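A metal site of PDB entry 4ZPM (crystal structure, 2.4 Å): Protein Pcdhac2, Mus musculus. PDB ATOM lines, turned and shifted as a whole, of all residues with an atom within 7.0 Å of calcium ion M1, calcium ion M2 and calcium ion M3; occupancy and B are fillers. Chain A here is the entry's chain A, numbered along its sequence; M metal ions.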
ATOM      1  N   GLU A 117      35.380   5.421 -25.388  1.00  0.00           N
ATOM      2  CA  GLU A 117      35.363   4.425 -26.448  1.00  0.00           C
ATOM      3  C   GLU A 117      34.546   4.878 -27.658  1.00  0.00           C
ATOM      4  O   GLU A 117      34.772   4.432 -28.777  1.00  0.00           O
ATOM      5  CB  GLU A 117      34.795   3.115 -25.895  1.00  0.00           C
ATOM      6  CG  GLU A 117      35.021   1.904 -26.738  1.00  0.00           C
ATOM      7  CD  GLU A 117      34.309   0.694 -26.188  1.00  0.00           C
ATOM      8  OE1 GLU A 117      33.695   0.818 -25.097  1.00  0.00           O
ATOM      9  OE2 GLU A 117      34.351  -0.370 -26.823  1.00  0.00           O
ATOM     10  N   LEU A 173      38.754   3.113 -30.779  1.00  0.00           N
ATOM     11  CA  LEU A 173      39.113   2.424 -29.541  1.00  0.00           C
ATOM     12  C   LEU A 173      38.041   1.418 -29.166  1.00  0.00           C
ATOM     13  O   LEU A 173      36.858   1.603 -29.470  1.00  0.00           O
ATOM     14  CB  LEU A 173      39.311   3.428 -28.408  1.00  0.00           C
ATOM     15  CG  LEU A 173      40.441   4.454 -28.591  1.00  0.00           C
ATOM     16  CD1 LEU A 173      40.502   5.388 -27.388  1.00  0.00           C
ATOM     17  CD2 LEU A 173      41.778   3.758 -28.799  1.00  0.00           C
ATOM     18  N   ASP A 174      38.452   0.337 -28.522  1.00  0.00           N
ATOM     19  CA  ASP A 174      37.519  -0.682 -28.056  1.00  0.00           C
ATOM     20  C   ASP A 174      37.953  -1.209 -26.698  1.00  0.00           C
ATOM     21  O   ASP A 174      38.874  -2.016 -26.604  1.00  0.00           O
ATOM     22  CB  ASP A 174      37.419  -1.828 -29.064  1.00  0.00           C
ATOM     23  CG  ASP A 174      36.421  -2.895 -28.665  1.00  0.00           C
ATOM     24  OD1 ASP A 174      35.615  -2.653 -27.732  1.00  0.00           O
ATOM     25  OD2 ASP A 174      36.441  -3.987 -29.278  1.00  0.00           O
ATOM     26  N   ARG A 175      37.286  -0.740 -25.645  1.00  0.00           N
ATOM     27  CA  ARG A 175      37.657  -1.087 -24.278  1.00  0.00           C
ATOM     28  C   ARG A 175      37.560  -2.599 -24.026  1.00  0.00           C
ATOM     29  O   ARG A 175      38.337  -3.154 -23.238  1.00  0.00           O
ATOM     30  CB  ARG A 175      36.773  -0.347 -23.270  1.00  0.00           C
ATOM     31  CG  ARG A 175      37.136  -0.631 -21.833  1.00  0.00           C
ATOM     32  CD  ARG A 175      35.952  -0.461 -20.907  1.00  0.00           C
ATOM     33  NE  ARG A 175      34.983  -1.535 -21.099  1.00  0.00           N
ATOM     34  CZ  ARG A 175      35.094  -2.755 -20.580  1.00  0.00           C
ATOM     35  NH1 ARG A 175      36.146  -3.062 -19.835  1.00  0.00           N
ATOM     36  NH2 ARG A 175      34.152  -3.660 -20.806  1.00  0.00           N
ATOM     37  N   GLU A 176      36.610  -3.247 -24.679  1.00  0.00           N
ATOM     38  CA  GLU A 176      36.431  -4.694 -24.536  1.00  0.00           C
ATOM     39  C   GLU A 176      37.623  -5.442 -25.124  1.00  0.00           C
ATOM     40  O   GLU A 176      37.965  -6.533 -24.666  1.00  0.00           O
ATOM     41  CB  GLU A 176      35.135  -5.138 -25.207  1.00  0.00           C
ATOM     42  CG  GLU A 176      33.909  -4.789 -24.392  1.00  0.00           C
ATOM     43  CD  GLU A 176      33.480  -3.345 -24.565  1.00  0.00           C
ATOM     44  OE1 GLU A 176      33.023  -2.738 -23.579  1.00  0.00           O
ATOM     45  OE2 GLU A 176      33.617  -2.809 -25.684  1.00  0.00           O
ATOM     46  N   GLN A 177      38.245  -4.846 -26.132  1.00  0.00           N
ATOM     47  CA  GLN A 177      39.480  -5.372 -26.698  1.00  0.00           C
ATOM     48  C   GLN A 177      40.676  -4.969 -25.823  1.00  0.00           C
ATOM     49  O   GLN A 177      41.430  -5.824 -25.370  1.00  0.00           O
ATOM     50  CB  GLN A 177      39.674  -4.870 -28.131  1.00  0.00           C
ATOM     51  CG  GLN A 177      40.752  -5.592 -28.910  1.00  0.00           C
ATOM     52  CD  GLN A 177      40.446  -5.658 -30.390  1.00  0.00           C
ATOM     53  OE1 GLN A 177      39.383  -5.228 -30.847  1.00  0.00           O
ATOM     54  NE2 GLN A 177      41.390  -6.196 -31.163  1.00  0.00           N
ATOM     55  N   LEU A 206      37.470   4.629 -21.736  1.00  0.00           N
ATOM     56  CA  LEU A 206      36.284   4.578 -20.896  1.00  0.00           C
ATOM     57  C   LEU A 206      35.193   3.780 -21.582  1.00  0.00           C
ATOM     58  O   LEU A 206      35.079   3.798 -22.803  1.00  0.00           O
ATOM     59  CB  LEU A 206      35.797   5.996 -20.581  1.00  0.00           C
ATOM     60  CG  LEU A 206      36.821   6.941 -19.954  1.00  0.00           C
ATOM     61  CD1 LEU A 206      36.205   8.309 -19.685  1.00  0.00           C
ATOM     62  CD2 LEU A 206      37.397   6.349 -18.672  1.00  0.00           C
ATOM     63  N   ASP A 207      34.383   3.078 -20.786  1.00  0.00           N
ATOM     64  CA  ASP A 207      33.359   2.199 -21.332  1.00  0.00           C
ATOM     65  C   ASP A 207      32.135   2.955 -21.835  1.00  0.00           C
ATOM     66  O   ASP A 207      31.645   3.868 -21.165  1.00  0.00           O
ATOM     67  CB  ASP A 207      32.913   1.164 -20.288  1.00  0.00           C
ATOM     68  CG  ASP A 207      31.936   0.155 -20.844  1.00  0.00           C
ATOM     69  OD1 ASP A 207      32.199  -0.404 -21.926  1.00  0.00           O
ATOM     70  OD2 ASP A 207      30.886  -0.076 -20.205  1.00  0.00           O
ATOM     71  N   THR A 208      31.659   2.594 -23.017  1.00  0.00           N
ATOM     72  CA  THR A 208      30.341   3.015 -23.469  1.00  0.00           C
ATOM     73  C   THR A 208      29.472   1.777 -23.604  1.00  0.00           C
ATOM     74  O   THR A 208      29.977   0.659 -23.741  1.00  0.00           O
ATOM     75  CB  THR A 208      30.388   3.769 -24.807  1.00  0.00           C
ATOM     76  OG1 THR A 208      30.669   2.839 -25.864  1.00  0.00           O
ATOM     77  CG2 THR A 208      31.457   4.850 -24.783  1.00  0.00           C
ATOM     78  N   ASN A 209      28.158   1.965 -23.561  1.00  0.00           N
ATOM     79  CA  ASN A 209      27.239   0.841 -23.715  1.00  0.00           C
ATOM     80  C   ASN A 209      27.031   0.519 -25.184  1.00  0.00           C
ATOM     81  O   ASN A 209      25.954   0.758 -25.735  1.00  0.00           O
ATOM     82  CB  ASN A 209      25.897   1.155 -23.039  1.00  0.00           C
ATOM     83  CG  ASN A 209      25.083  -0.085 -22.771  1.00  0.00           C
ATOM     84  OD1 ASN A 209      25.406  -1.168 -23.247  1.00  0.00           O
ATOM     85  ND2 ASN A 209      24.000   0.072 -22.010  1.00  0.00           N
ATOM     86  N   ASP A 210      28.055  -0.037 -25.816  1.00  0.00           N
ATOM     87  CA  ASP A 210      28.036  -0.266 -27.255  1.00  0.00           C
ATOM     88  C   ASP A 210      27.854  -1.746 -27.612  1.00  0.00           C
ATOM     89  O   ASP A 210      27.958  -2.129 -28.775  1.00  0.00           O
ATOM     90  CB  ASP A 210      29.309   0.266 -27.903  1.00  0.00           C
ATOM     91  CG  ASP A 210      30.567  -0.388 -27.360  1.00  0.00           C
ATOM     92  OD1 ASP A 210      30.503  -0.995 -26.267  1.00  0.00           O
ATOM     93  OD2 ASP A 210      31.626  -0.294 -28.025  1.00  0.00           O
ATOM     94  N   ASN A 211      27.551  -2.561 -26.600  1.00  0.00           N
ATOM     95  CA  ASN A 211      27.255  -3.972 -26.815  1.00  0.00           C
ATOM     96  C   ASN A 211      25.886  -4.325 -26.256  1.00  0.00           C
ATOM     97  O   ASN A 211      25.564  -3.975 -25.118  1.00  0.00           O
ATOM     98  CB  ASN A 211      28.329  -4.858 -26.174  1.00  0.00           C
ATOM     99  CG  ASN A 211      29.632  -4.867 -26.950  1.00  0.00           C
ATOM    100  OD1 ASN A 211      29.824  -5.693 -27.846  1.00  0.00           O
ATOM    101  ND2 ASN A 211      30.524  -3.956 -26.610  1.00  0.00           N
ATOM    102  N   SER A 212      25.086  -5.018 -27.050  1.00  0.00           N
ATOM    103  CA  SER A 212      23.787  -5.486 -26.593  1.00  0.00           C
ATOM    104  C   SER A 212      23.892  -6.932 -26.129  1.00  0.00           C
ATOM    105  O   SER A 212      24.698  -7.691 -26.663  1.00  0.00           O
ATOM    106  CB  SER A 212      22.744  -5.340 -27.710  1.00  0.00           C
ATOM    107  OG  SER A 212      23.237  -5.816 -28.939  1.00  0.00           O
ATOM    108  N   PRO A 213      23.092  -7.308 -25.119  1.00  0.00           N
ATOM    109  CA  PRO A 213      23.052  -8.670 -24.583  1.00  0.00           C
ATOM    110  C   PRO A 213      22.850  -9.706 -25.670  1.00  0.00           C
ATOM    111  O   PRO A 213      22.168  -9.434 -26.649  1.00  0.00           O
ATOM    112  CB  PRO A 213      21.850  -8.641 -23.636  1.00  0.00           C
ATOM    113  CG  PRO A 213      21.744  -7.214 -23.220  1.00  0.00           C
ATOM    114  CD  PRO A 213      22.167  -6.402 -24.406  1.00  0.00           C
ATOM    115  N   ASP A 241      27.033 -10.048 -21.664  1.00  0.00           N
ATOM    116  CA  ASP A 241      27.296  -8.695 -22.127  1.00  0.00           C
ATOM    117  C   ASP A 241      28.715  -8.265 -21.750  1.00  0.00           C
ATOM    118  O   ASP A 241      29.019  -8.101 -20.566  1.00  0.00           O
ATOM    119  CB  ASP A 241      26.272  -7.718 -21.536  1.00  0.00           C
ATOM    120  CG  ASP A 241      26.222  -6.405 -22.298  1.00  0.00           C
ATOM    121  OD1 ASP A 241      27.110  -5.548 -22.083  1.00  0.00           O
ATOM    122  OD2 ASP A 241      25.282  -6.211 -23.094  1.00  0.00           O
ATOM    123  N   PRO A 242      29.583  -8.055 -22.749  1.00  0.00           N
ATOM    124  CA  PRO A 242      31.005  -7.787 -22.530  1.00  0.00           C
ATOM    125  C   PRO A 242      31.321  -6.387 -22.000  1.00  0.00           C
ATOM    126  O   PRO A 242      32.469  -6.128 -21.655  1.00  0.00           O
ATOM    127  CB  PRO A 242      31.616  -7.978 -23.920  1.00  0.00           C
ATOM    128  CG  PRO A 242      30.501  -7.641 -24.857  1.00  0.00           C
ATOM    129  CD  PRO A 242      29.248  -8.116 -24.183  1.00  0.00           C
ATOM    130  N   ASP A 243      30.322  -5.505 -21.925  1.00  0.00           N
ATOM    131  CA  ASP A 243      30.557  -4.149 -21.433  1.00  0.00           C
ATOM    132  C   ASP A 243      30.867  -4.149 -19.931  1.00  0.00           C
ATOM    133  O   ASP A 243      30.803  -5.186 -19.280  1.00  0.00           O
ATOM    134  CB  ASP A 243      29.353  -3.258 -21.718  1.00  0.00           C
ATOM    135  CG  ASP A 243      29.200  -2.956 -23.202  1.00  0.00           C
ATOM    136  OD1 ASP A 243      30.196  -3.096 -23.941  1.00  0.00           O
ATOM    137  OD2 ASP A 243      28.086  -2.575 -23.630  1.00  0.00           O
ATOM    138  N   GLU A 244      31.198  -2.972 -19.401  1.00  0.00           N
ATOM    139  CA  GLU A 244      31.704  -2.871 -18.045  1.00  0.00           C
ATOM    140  C   GLU A 244      30.658  -2.401 -17.042  1.00  0.00           C
ATOM    141  O   GLU A 244      29.885  -1.473 -17.314  1.00  0.00           O
ATOM    142  CB  GLU A 244      32.896  -1.911 -18.008  1.00  0.00           C
ATOM    143  CG  GLU A 244      33.436  -1.608 -16.619  1.00  0.00           C
ATOM    144  CD  GLU A 244      34.595  -0.621 -16.645  1.00  0.00           C
ATOM    145  OE1 GLU A 244      34.440   0.469 -17.243  1.00  0.00           O
ATOM    146  OE2 GLU A 244      35.656  -0.939 -16.072  1.00  0.00           O
ATOM    147  N   SER A 246      27.594  -1.617 -14.859  1.00  0.00           N
ATOM    148  CA  SER A 246      26.161  -1.519 -15.081  1.00  0.00           C
ATOM    149  C   SER A 246      25.789  -1.752 -16.545  1.00  0.00           C
ATOM    150  O   SER A 246      24.698  -2.222 -16.843  1.00  0.00           O
ATOM    151  CB  SER A 246      25.646  -0.158 -14.617  1.00  0.00           C
ATOM    152  OG  SER A 246      24.269   0.003 -14.912  1.00  0.00           O
ATOM    153  N   ASN A 247      26.707  -1.407 -17.444  1.00  0.00           N
ATOM    154  CA  ASN A 247      26.477  -1.582 -18.880  1.00  0.00           C
ATOM    155  C   ASN A 247      26.481  -3.043 -19.330  1.00  0.00           C
ATOM    156  O   ASN A 247      25.984  -3.367 -20.409  1.00  0.00           O
ATOM    157  CB  ASN A 247      27.523  -0.809 -19.675  1.00  0.00           C
ATOM    158  CG  ASN A 247      27.438   0.679 -19.430  1.00  0.00           C
ATOM    159  OD1 ASN A 247      26.445   1.320 -19.777  1.00  0.00           O
ATOM    160  ND2 ASN A 247      28.489   1.242 -18.836  1.00  0.00           N
ATOM    161  N   GLY A 248      27.065  -3.915 -18.514  1.00  0.00           N
ATOM    162  CA  GLY A 248      27.105  -5.340 -18.839  1.00  0.00           C
ATOM    163  C   GLY A 248      26.248  -6.184 -17.905  1.00  0.00           C
ATOM    164  O   GLY A 248      26.354  -7.409 -17.901  1.00  0.00           O
ATOM    165  N   GLU A 249      25.375  -5.531 -17.148  1.00  0.00           N
ATOM    166  CA  GLU A 249      24.555  -6.231 -16.170  1.00  0.00           C
ATOM    167  C   GLU A 249      23.172  -6.482 -16.756  1.00  0.00           C
ATOM    168  O   GLU A 249      22.520  -5.566 -17.252  1.00  0.00           O
ATOM    169  CB  GLU A 249      24.463  -5.434 -14.869  1.00  0.00           C
ATOM    170  CG  GLU A 249      25.470  -5.881 -13.821  1.00  0.00           C
ATOM    171  CD  GLU A 249      24.857  -6.020 -12.446  1.00  0.00           C
ATOM    172  OE1 GLU A 249      23.889  -5.296 -12.142  1.00  0.00           O
ATOM    173  OE2 GLU A 249      25.342  -6.875 -11.662  1.00  0.00           O
ATOM    174  N   LEU A 250      22.739  -7.738 -16.682  1.00  0.00           N
ATOM    175  CA  LEU A 250      21.551  -8.182 -17.395  1.00  0.00           C
ATOM    176  C   LEU A 250      20.360  -8.475 -16.484  1.00  0.00           C
ATOM    177  O   LEU A 250      20.521  -8.946 -15.361  1.00  0.00           O
ATOM    178  CB  LEU A 250      21.880  -9.423 -18.224  1.00  0.00           C
ATOM    179  CG  LEU A 250      23.113  -9.265 -19.115  1.00  0.00           C
ATOM    180  CD1 LEU A 250      23.333 -10.491 -19.978  1.00  0.00           C
ATOM    181  CD2 LEU A 250      22.994  -8.016 -19.971  1.00  0.00           C
ATOM    182  N   ASP A 297      20.180  -4.502 -20.811  1.00  0.00           N
ATOM    183  CA  ASP A 297      21.244  -3.809 -20.072  1.00  0.00           C
ATOM    184  C   ASP A 297      20.705  -2.994 -18.920  1.00  0.00           C
ATOM    185  O   ASP A 297      19.509  -2.710 -18.851  1.00  0.00           O
ATOM    186  CB  ASP A 297      22.030  -2.878 -21.003  1.00  0.00           C
ATOM    187  CG  ASP A 297      22.978  -3.624 -21.905  1.00  0.00           C
ATOM    188  OD1 ASP A 297      23.274  -4.799 -21.607  1.00  0.00           O
ATOM    189  OD2 ASP A 297      23.409  -3.043 -22.915  1.00  0.00           O
ATOM    190  N   ARG A 298      21.592  -2.610 -18.015  1.00  0.00           N
ATOM    191  CA  ARG A 298      21.290  -1.617 -16.994  1.00  0.00           C
ATOM    192  C   ARG A 298      22.039  -0.315 -17.285  1.00  0.00           C
ATOM    193  O   ARG A 298      22.217   0.517 -16.404  1.00  0.00           O
ATOM    194  CB  ARG A 298      21.645  -2.134 -15.601  1.00  0.00           C
ATOM    195  CG  ARG A 298      20.663  -3.138 -15.034  1.00  0.00           C
ATOM    196  CD  ARG A 298      21.067  -3.567 -13.626  1.00  0.00           C
ATOM    197  N   GLY A 299      22.475  -0.155 -18.531  1.00  0.00           N
ATOM    198  CA  GLY A 299      23.152   1.057 -18.943  1.00  0.00           C
ATOM    199  C   GLY A 299      22.207   2.240 -19.085  1.00  0.00           C
ATOM    200  O   GLY A 299      20.993   2.081 -18.975  1.00  0.00           O
ATOM    201  N   VAL A 301      21.421   4.036 -21.749  1.00  0.00           N
ATOM    202  CA  VAL A 301      20.514   3.620 -22.816  1.00  0.00           C
ATOM    203  C   VAL A 301      20.486   2.101 -22.849  1.00  0.00           C
ATOM    204  O   VAL A 301      21.376   1.474 -23.421  1.00  0.00           O
ATOM    205  CB  VAL A 301      20.948   4.164 -24.190  1.00  0.00           C
ATOM    206  CG1 VAL A 301      19.986   3.710 -25.272  1.00  0.00           C
ATOM    207  CG2 VAL A 301      21.068   5.681 -24.150  1.00  0.00           C
ATOM    208  N   MET A 303      20.184  -1.683 -23.637  1.00  0.00           N
ATOM    209  CA  MET A 303      20.260  -2.401 -24.892  1.00  0.00           C
ATOM    210  C   MET A 303      19.756  -3.815 -24.650  1.00  0.00           C
ATOM    211  O   MET A 303      19.894  -4.332 -23.545  1.00  0.00           O
ATOM    212  CB  MET A 303      21.689  -2.436 -25.424  1.00  0.00           C
ATOM    213  CG  MET A 303      22.301  -1.065 -25.670  1.00  0.00           C
ATOM    214  SD  MET A 303      21.802  -0.350 -27.248  1.00  0.00           S
ATOM    215  CE  MET A 303      22.419   1.327 -27.060  1.00  0.00           C
HETATM  216 CA    CA M   1      33.335  -1.875 -28.157  1.00  0.00          CA
HETATM  217 CA    CA M   2      31.673  -0.963 -24.198  1.00  0.00          CA
HETATM  218 CA    CA M   3      25.804  -3.601 -22.837  1.00  0.00          CA
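O of Leu 206 sits at hydrogen-bond distance from N of Glu 117 (3.1 Å).
OE1 of Glu 176 lies close to NH2 of Arg 175, at 3.1 Å.
The side-chain amide nitrogen of Asn 211 sits close to the side-chain carboxylate of Asp 210 (3.0 Å).
The side-chain amide nitrogen (ND2) of Asn 247 sits at hydrogen-bond distance from the side-chain carboxylate (OD2) of Asp 207 (3.1 Å).
OD1 of Asp 207 lies close to NE of Arg 175, 3.1 Å away.
OD2 of Asp 207 lies within hydrogen-bond range of N of Glu 244, 3.0 Å away.
The side-chain amide nitrogen (ND2) of Asn 247 sits close to the backbone carbonyl oxygen (O) of Glu 244 (3.4 Å).
ND2 of Asn 209 sits at hydrogen-bond distance from O of Val 301 (3.3 Å).
Calcium ion M1 is bound by OE2 of Glu 117, OD2 of Asp 210, OD1 of Asp 174 and OE2 of Glu 176.
Calcium ion M1 has four donor atoms within binding distance.
Six residues have an atom within 4 Å of calcium ion M3: Asn 209, Asn 211, Asp 241, Asp 243, Asn 247 and Asp 297.
The nearest printed residue that does not touch calcium ion M3 is Ser 212 (4.5 Å).
Calcium ion M2 is bound by the side-chain carboxylate (OE1) of Glu 176 (2.3 Å), the side-chain carboxylate (OD1) of Asp 210 (2.4 Å), the backbone carbonyl oxygen (O) of Thr 208 (2.4 Å), the side-chain carboxylate (OD1) of Asp 207 (2.4 Å), the side-chain carboxylate (OD1) of Asp 243 (2.6 Å) and the side-chain carboxylate (OE1) of Glu 117 (2.8 Å).
Calcium ion M2 has six donor atoms within binding distance.
Slightly farther from calcium ion M2 lies the side-chain carboxylate (OE2) of Glu 176 (3.1 Å).
Calcium ion M3 is bound by the backbone carbonyl oxygen (O) of Asn 211 (2.3 Å), the backbone carbonyl oxygen (O) of Asn 247 (2.4 Å), the side-chain carboxylate (OD2) of Asp 297 (2.5 Å), the side-chain carboxylate (OD1) of Asp 241 (2.5 Å), the side-chain amide oxygen (OD1) of Asn 209 (2.5 Å), the side-chain carboxylate (OD2) of Asp 243 (2.6 Å) and the side-chain carboxylate (OD2) of Asp 241 (2.7 Å).
Slightly farther from calcium ion M3 lies OD1 of Asp 297 (3.1 Å).
Along chain A the residues within 4 Å of calcium ion M2 span positions 117 to 243.
The nearest printed residue that does not touch calcium ion M2 is Asn 211 (4.01 Å).
Of the 28 residues printed, 5 come within 4 Å of calcium ion M1.
The nearest printed residue that does not touch calcium ion M1 is Arg 175 (4.8 Å).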
